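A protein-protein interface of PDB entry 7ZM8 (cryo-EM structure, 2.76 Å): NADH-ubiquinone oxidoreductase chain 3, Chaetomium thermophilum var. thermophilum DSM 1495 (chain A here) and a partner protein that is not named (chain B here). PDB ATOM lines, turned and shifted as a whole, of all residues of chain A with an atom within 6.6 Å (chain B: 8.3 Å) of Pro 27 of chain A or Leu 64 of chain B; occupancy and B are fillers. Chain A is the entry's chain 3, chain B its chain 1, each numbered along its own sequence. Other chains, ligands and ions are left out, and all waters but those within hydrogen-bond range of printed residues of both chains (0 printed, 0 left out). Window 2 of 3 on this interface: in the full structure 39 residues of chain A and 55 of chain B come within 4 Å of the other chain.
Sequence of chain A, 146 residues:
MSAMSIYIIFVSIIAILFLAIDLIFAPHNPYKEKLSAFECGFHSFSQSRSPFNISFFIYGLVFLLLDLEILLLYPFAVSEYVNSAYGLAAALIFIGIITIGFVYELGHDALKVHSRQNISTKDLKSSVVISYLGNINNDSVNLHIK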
ATOM      1  N   ILE A  21     -17.671 -32.793   3.752  1.00  0.00           N
ATOM      2  CA  ILE A  21     -18.663 -33.189   2.758  1.00  0.00           C
ATOM      3  C   ILE A  21     -18.925 -32.048   1.782  1.00  0.00           C
ATOM      4  O   ILE A  21     -19.079 -32.264   0.573  1.00  0.00           O
ATOM      5  CB  ILE A  21     -19.957 -33.650   3.452  1.00  0.00           C
ATOM      6  CG1 ILE A  21     -19.650 -34.732   4.490  1.00  0.00           C
ATOM      7  CG2 ILE A  21     -20.964 -34.157   2.433  1.00  0.00           C
ATOM      8  CD1 ILE A  21     -18.977 -35.957   3.913  1.00  0.00           C
ATOM      9  N   ASP A  22     -18.974 -30.815   2.288  1.00  0.00           N
ATOM     10  CA  ASP A  22     -19.169 -29.668   1.412  1.00  0.00           C
ATOM     11  C   ASP A  22     -17.994 -29.492   0.459  1.00  0.00           C
ATOM     12  O   ASP A  22     -18.183 -29.317  -0.750  1.00  0.00           O
ATOM     13  CB  ASP A  22     -19.378 -28.404   2.246  1.00  0.00           C
ATOM     14  CG  ASP A  22     -19.196 -27.141   1.437  1.00  0.00           C
ATOM     15  OD1 ASP A  22     -20.095 -26.819   0.635  1.00  0.00           O
ATOM     16  OD2 ASP A  22     -18.152 -26.474   1.593  1.00  0.00           O
ATOM     17  N   PHE A  25     -17.751 -32.868  -1.899  1.00  0.00           N
ATOM     18  CA  PHE A  25     -18.851 -33.273  -2.767  1.00  0.00           C
ATOM     19  C   PHE A  25     -19.617 -32.124  -3.402  1.00  0.00           C
ATOM     20  O   PHE A  25     -20.002 -32.230  -4.569  1.00  0.00           O
ATOM     21  CB  PHE A  25     -19.832 -34.155  -1.989  1.00  0.00           C
ATOM     22  CG  PHE A  25     -19.361 -35.569  -1.811  1.00  0.00           C
ATOM     23  CD1 PHE A  25     -18.761 -36.248  -2.858  1.00  0.00           C
ATOM     24  CD2 PHE A  25     -19.517 -36.218  -0.600  1.00  0.00           C
ATOM     25  CE1 PHE A  25     -18.326 -37.549  -2.700  1.00  0.00           C
ATOM     26  CE2 PHE A  25     -19.084 -37.520  -0.435  1.00  0.00           C
ATOM     27  CZ  PHE A  25     -18.488 -38.186  -1.486  1.00  0.00           C
ATOM     28  N   ALA A  26     -19.860 -31.038  -2.679  1.00  0.00           N
ATOM     29  CA  ALA A  26     -20.675 -29.961  -3.222  1.00  0.00           C
ATOM     30  C   ALA A  26     -19.989 -29.352  -4.442  1.00  0.00           C
ATOM     31  O   ALA A  26     -18.756 -29.311  -4.505  1.00  0.00           O
ATOM     32  CB  ALA A  26     -20.925 -28.886  -2.165  1.00  0.00           C
ATOM     33  N   PRO A  27     -20.747 -28.896  -5.435  1.00  0.00           N
ATOM     34  CA  PRO A  27     -20.123 -28.340  -6.639  1.00  0.00           C
ATOM     35  C   PRO A  27     -19.353 -27.068  -6.330  1.00  0.00           C
ATOM     36  O   PRO A  27     -19.665 -26.333  -5.389  1.00  0.00           O
ATOM     37  CB  PRO A  27     -21.314 -28.054  -7.560  1.00  0.00           C
ATOM     38  CG  PRO A  27     -22.443 -28.864  -7.003  1.00  0.00           C
ATOM     39  CD  PRO A  27     -22.214 -28.907  -5.530  1.00  0.00           C
ATOM     40  N   HIS A  28     -18.328 -26.817  -7.139  1.00  0.00           N
ATOM     41  CA  HIS A  28     -17.483 -25.644  -6.985  1.00  0.00           C
ATOM     42  C   HIS A  28     -17.292 -24.967  -8.333  1.00  0.00           C
ATOM     43  O   HIS A  28     -17.231 -25.634  -9.370  1.00  0.00           O
ATOM     44  CB  HIS A  28     -16.125 -26.019  -6.398  1.00  0.00           C
ATOM     45  CG  HIS A  28     -16.193 -26.483  -4.978  1.00  0.00           C
ATOM     46  ND1 HIS A  28     -16.466 -27.788  -4.632  1.00  0.00           N
ATOM     47  CD2 HIS A  28     -16.022 -25.813  -3.814  1.00  0.00           C
ATOM     48  CE1 HIS A  28     -16.459 -27.903  -3.317  1.00  0.00           C
ATOM     49  NE2 HIS A  28     -16.191 -26.720  -2.796  1.00  0.00           N
ATOM     50  N   ASN A  29     -17.204 -23.639  -8.312  1.00  0.00           N
ATOM     51  CA  ASN A  29     -16.940 -22.860  -9.511  1.00  0.00           C
ATOM     52  C   ASN A  29     -15.810 -21.880  -9.221  1.00  0.00           C
ATOM     53  O   ASN A  29     -15.825 -21.212  -8.171  1.00  0.00           O
ATOM     54  CB  ASN A  29     -18.193 -22.109  -9.977  1.00  0.00           C
ATOM     55  CG  ASN A  29     -19.215 -23.026 -10.613  1.00  0.00           C
ATOM     56  OD1 ASN A  29     -18.868 -23.924 -11.379  1.00  0.00           O
ATOM     57  ND2 ASN A  29     -20.487 -22.804 -10.299  1.00  0.00           N
ATOM     58  N   PHE B  56     -33.287 -35.663   7.367  1.00  0.00           N
ATOM     59  CA  PHE B  56     -32.078 -36.202   6.758  1.00  0.00           C
ATOM     60  C   PHE B  56     -31.914 -35.720   5.325  1.00  0.00           C
ATOM     61  O   PHE B  56     -30.809 -35.358   4.911  1.00  0.00           O
ATOM     62  CB  PHE B  56     -32.109 -37.726   6.817  1.00  0.00           C
ATOM     63  CG  PHE B  56     -31.768 -38.281   8.164  1.00  0.00           C
ATOM     64  CD1 PHE B  56     -32.573 -38.022   9.259  1.00  0.00           C
ATOM     65  CD2 PHE B  56     -30.628 -39.046   8.344  1.00  0.00           C
ATOM     66  CE1 PHE B  56     -32.256 -38.524  10.505  1.00  0.00           C
ATOM     67  CE2 PHE B  56     -30.305 -39.551   9.587  1.00  0.00           C
ATOM     68  CZ  PHE B  56     -31.120 -39.291  10.668  1.00  0.00           C
ATOM     69  N   ALA B  57     -33.000 -35.717   4.553  1.00  0.00           N
ATOM     70  CA  ALA B  57     -32.930 -35.245   3.176  1.00  0.00           C
ATOM     71  C   ALA B  57     -32.608 -33.762   3.117  1.00  0.00           C
ATOM     72  O   ALA B  57     -31.787 -33.331   2.301  1.00  0.00           O
ATOM     73  CB  ALA B  57     -34.243 -35.534   2.456  1.00  0.00           C
ATOM     74  N   ASP B  58     -33.246 -32.966   3.972  1.00  0.00           N
ATOM     75  CA  ASP B  58     -33.005 -31.529   3.969  1.00  0.00           C
ATOM     76  C   ASP B  58     -31.585 -31.210   4.405  1.00  0.00           C
ATOM     77  O   ASP B  58     -30.944 -30.313   3.846  1.00  0.00           O
ATOM     78  CB  ASP B  58     -34.016 -30.829   4.872  1.00  0.00           C
ATOM     79  CG  ASP B  58     -35.448 -31.065   4.436  1.00  0.00           C
ATOM     80  OD1 ASP B  58     -35.688 -31.217   3.219  1.00  0.00           O
ATOM     81  OD2 ASP B  58     -36.332 -31.104   5.316  1.00  0.00           O
ATOM     82  N   ALA B  59     -31.083 -31.920   5.414  1.00  0.00           N
ATOM     83  CA  ALA B  59     -29.706 -31.713   5.846  1.00  0.00           C
ATOM     84  C   ALA B  59     -28.720 -32.162   4.780  1.00  0.00           C
ATOM     85  O   ALA B  59     -27.704 -31.502   4.549  1.00  0.00           O
ATOM     86  CB  ALA B  59     -29.451 -32.454   7.158  1.00  0.00           C
ATOM     87  N   LEU B  60     -28.999 -33.290   4.129  1.00  0.00           N
ATOM     88  CA  LEU B  60     -28.108 -33.779   3.085  1.00  0.00           C
ATOM     89  C   LEU B  60     -28.192 -32.911   1.842  1.00  0.00           C
ATOM     90  O   LEU B  60     -27.183 -32.694   1.164  1.00  0.00           O
ATOM     91  CB  LEU B  60     -28.441 -35.231   2.755  1.00  0.00           C
ATOM     92  CG  LEU B  60     -27.550 -35.907   1.723  1.00  0.00           C
ATOM     93  CD1 LEU B  60     -26.122 -35.978   2.223  1.00  0.00           C
ATOM     94  CD2 LEU B  60     -28.079 -37.287   1.402  1.00  0.00           C
ATOM     95  N   LYS B  61     -29.385 -32.409   1.522  1.00  0.00           N
ATOM     96  CA  LYS B  61     -29.540 -31.571   0.339  1.00  0.00           C
ATOM     97  C   LYS B  61     -28.697 -30.312   0.446  1.00  0.00           C
ATOM     98  O   LYS B  61     -28.080 -29.886  -0.535  1.00  0.00           O
ATOM     99  CB  LYS B  61     -31.011 -31.217   0.141  1.00  0.00           C
ATOM    100  CG  LYS B  61     -31.336 -30.512  -1.162  1.00  0.00           C
ATOM    101  CD  LYS B  61     -31.344 -29.009  -1.001  1.00  0.00           C
ATOM    102  CE  LYS B  61     -32.434 -28.557  -0.059  1.00  0.00           C
ATOM    103  NZ  LYS B  61     -32.452 -27.077   0.044  1.00  0.00           N
ATOM    104  N   LEU B  62     -28.671 -29.695   1.625  1.00  0.00           N
ATOM    105  CA  LEU B  62     -27.863 -28.498   1.814  1.00  0.00           C
ATOM    106  C   LEU B  62     -26.380 -28.804   1.670  1.00  0.00           C
ATOM    107  O   LEU B  62     -25.631 -28.017   1.081  1.00  0.00           O
ATOM    108  CB  LEU B  62     -28.152 -27.881   3.179  1.00  0.00           C
ATOM    109  CG  LEU B  62     -29.452 -27.090   3.318  1.00  0.00           C
ATOM    110  CD1 LEU B  62     -29.510 -26.410   4.671  1.00  0.00           C
ATOM    111  CD2 LEU B  62     -29.586 -26.072   2.205  1.00  0.00           C
ATOM    112  N   LEU B  63     -25.940 -29.948   2.201  1.00  0.00           N
ATOM    113  CA  LEU B  63     -24.525 -30.298   2.176  1.00  0.00           C
ATOM    114  C   LEU B  63     -23.996 -30.423   0.757  1.00  0.00           C
ATOM    115  O   LEU B  63     -22.857 -30.033   0.483  1.00  0.00           O
ATOM    116  CB  LEU B  63     -24.304 -31.603   2.934  1.00  0.00           C
ATOM    117  CG  LEU B  63     -24.233 -31.493   4.453  1.00  0.00           C
ATOM    118  CD1 LEU B  63     -24.136 -32.868   5.054  1.00  0.00           C
ATOM    119  CD2 LEU B  63     -23.057 -30.642   4.857  1.00  0.00           C
ATOM    120  N   LEU B  64     -24.804 -30.954  -0.155  1.00  0.00           N
ATOM    121  CA  LEU B  64     -24.410 -31.161  -1.539  1.00  0.00           C
ATOM    122  C   LEU B  64     -24.716 -29.964  -2.420  1.00  0.00           C
ATOM    123  O   LEU B  64     -24.579 -30.058  -3.642  1.00  0.00           O
ATOM    124  CB  LEU B  64     -25.099 -32.403  -2.094  1.00  0.00           C
ATOM    125  CG  LEU B  64     -25.109 -33.600  -1.152  1.00  0.00           C
ATOM    126  CD1 LEU B  64     -25.948 -34.709  -1.742  1.00  0.00           C
ATOM    127  CD2 LEU B  64     -23.698 -34.076  -0.891  1.00  0.00           C
ATOM    128  N   LYS B  65     -25.136 -28.851  -1.838  1.00  0.00           N
ATOM    129  CA  LYS B  65     -25.454 -27.653  -2.595  1.00  0.00           C
ATOM    130  C   LYS B  65     -24.208 -26.805  -2.782  1.00  0.00           C
ATOM    131  O   LYS B  65     -23.383 -26.669  -1.877  1.00  0.00           O
ATOM    132  CB  LYS B  65     -26.535 -26.837  -1.886  1.00  0.00           C
ATOM    133  CG  LYS B  65     -27.005 -25.603  -2.623  1.00  0.00           C
ATOM    134  CD  LYS B  65     -27.820 -25.959  -3.851  1.00  0.00           C
ATOM    135  CE  LYS B  65     -29.068 -25.084  -3.958  1.00  0.00           C
ATOM    136  NZ  LYS B  65     -28.762 -23.629  -3.885  1.00  0.00           N
ATOM    137  N   GLU B  66     -24.079 -26.236  -3.974  1.00  0.00           N
ATOM    138  CA  GLU B  66     -22.992 -25.315  -4.246  1.00  0.00           C
ATOM    139  C   GLU B  66     -23.105 -24.089  -3.355  1.00  0.00           C
ATOM    140  O   GLU B  66     -24.193 -23.560  -3.124  1.00  0.00           O
ATOM    141  CB  GLU B  66     -23.006 -24.896  -5.713  1.00  0.00           C
ATOM    142  N   TYR B  67     -21.968 -23.636  -2.847  1.00  0.00           N
ATOM    143  CA  TYR B  67     -21.900 -22.423  -2.049  1.00  0.00           C
ATOM    144  C   TYR B  67     -21.255 -21.327  -2.883  1.00  0.00           C
ATOM    145  O   TYR B  67     -20.235 -21.558  -3.539  1.00  0.00           O
ATOM    146  CB  TYR B  67     -21.130 -22.657  -0.749  1.00  0.00           C
ATOM    147  CG  TYR B  67     -19.680 -23.026  -0.937  1.00  0.00           C
ATOM    148  CD1 TYR B  67     -19.295 -24.352  -1.063  1.00  0.00           C
ATOM    149  CD2 TYR B  67     -18.691 -22.050  -0.963  1.00  0.00           C
ATOM    150  CE1 TYR B  67     -17.971 -24.696  -1.228  1.00  0.00           C
ATOM    151  CE2 TYR B  67     -17.364 -22.384  -1.130  1.00  0.00           C
ATOM    152  CZ  TYR B  67     -17.009 -23.706  -1.261  1.00  0.00           C
ATOM    153  OH  TYR B  67     -15.684 -24.037  -1.423  1.00  0.00           O
ATOM    154  N   VAL B  68     -21.868 -20.148  -2.875  1.00  0.00           N
ATOM    155  CA  VAL B  68     -21.428 -19.036  -3.701  1.00  0.00           C
ATOM    156  C   VAL B  68     -20.668 -17.993  -2.872  1.00  0.00           C
ATOM    157  O   VAL B  68     -20.585 -16.828  -3.260  1.00  0.00           O
ATOM    158  CB  VAL B  68     -22.612 -18.415  -4.465  1.00  0.00           C
ATOM    159  CG1 VAL B  68     -23.492 -17.562  -3.545  1.00  0.00           C
ATOM    160  CG2 VAL B  68     -22.141 -17.641  -5.701  1.00  0.00           C
ATOM    161  N   ILE B 228     -26.261 -22.585   2.052  1.00  0.00           N
ATOM    162  CA  ILE B 228     -25.930 -24.004   1.947  1.00  0.00           C
ATOM    163  C   ILE B 228     -25.485 -24.563   3.290  1.00  0.00           C
ATOM    164  O   ILE B 228     -25.340 -25.779   3.448  1.00  0.00           O
ATOM    165  CB  ILE B 228     -24.847 -24.236   0.878  1.00  0.00           C
ATOM    166  N   VAL B 230     -25.782 -25.969   6.727  1.00  0.00           N
ATOM    167  CA  VAL B 230     -26.580 -26.559   7.789  1.00  0.00           C
ATOM    168  C   VAL B 230     -26.099 -26.144   9.165  1.00  0.00           C
ATOM    169  O   VAL B 230     -26.803 -26.374  10.154  1.00  0.00           O
ATOM    170  CB  VAL B 230     -26.556 -28.100   7.720  1.00  0.00           C
ATOM    171  CG1 VAL B 230     -27.148 -28.589   6.429  1.00  0.00           C
ATOM    172  CG2 VAL B 230     -25.131 -28.607   7.869  1.00  0.00           C
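The backbone carbonyl oxygen (O) of Ala 26 of chain A sits at hydrogen-bond distance from a ring nitrogen (ND1) of His 28 of chain A (2.8 Å).
Of the printed residues of chain B, Asp 22 of chain A touches Leu 63 (3.8 Å) and Tyr 67 (3.1 Å). Phe 25 of chain A touches none of the printed residues of chain B. Of the printed residues of chain B, Pro 27 of chain A touches Leu 64 (3.2 Å), Lys 65 (3.99 Å) and Glu 66 (3.6 Å). Ala 59 of chain B touches none of the printed residues of chain A. Printed residues of chain A within 4 Å of Leu 63 of chain B: Asp 22 and Ala 26. Printed residues of chain A within 4 Å of Leu 64 of chain B: Ala 26 (3.9 Å) and Pro 27 (3.2 Å). Printed residues of chain A within 4 Å of Lys 65 of chain B: Ala 26 (3.3 Å) and Pro 27 (3.99 Å). Of the printed residues of chain A, Tyr 67 of chain B touches Asp 22 (3.1 Å) and His 28 (3.0 Å). The nearest printed residue of chain B that does not touch Pro 27 of chain A is Tyr 67 of chain B (4.4 Å). The nearest printed residue of chain A that does not touch Leu 64 of chain B is Phe 25 of chain A (4.02 Å). The nearest printed residue of chain A that does not touch Leu 63 of chain B is Ile 21 of chain A (4.2 Å).
OH of Tyr 67 of chain B sits close to NE2 of His 28 of chain A, 3.1 Å away.
Among the printed residues, pairs that only touch across the chains: Asp 22 of chain A with Leu 63 of chain B (3.8 Å), Asp 22 of chain A with Tyr 67 of chain B (3.1 Å), Ala 26 of chain A with Leu 63 of chain B (3.5 Å), Ala 26 of chain A with Leu 64 of chain B (3.9 Å), Ala 26 of chain A with Lys 65 of chain B (3.3 Å), Pro 27 of chain A with Leu 64 of chain B (3.2 Å), Pro 27 of chain A with Lys 65 of chain B (3.99 Å) and Pro 27 of chain A with Glu 66 of chain B (3.6 Å).
Hydrophobic or aromatic side chains of chain B that line the printed part of chain A: Tyr 67. Printed residues of chain A that touch a printed residue of chain B: Asp 22, Ala 26, Pro 27 and His 28. Hydrophobic or aromatic side chains of chain A within 4 Å of the printed part of chain B: Ala 26, Pro 27 and His 28. Among the printed residues, 9 pairs touch across the chains.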
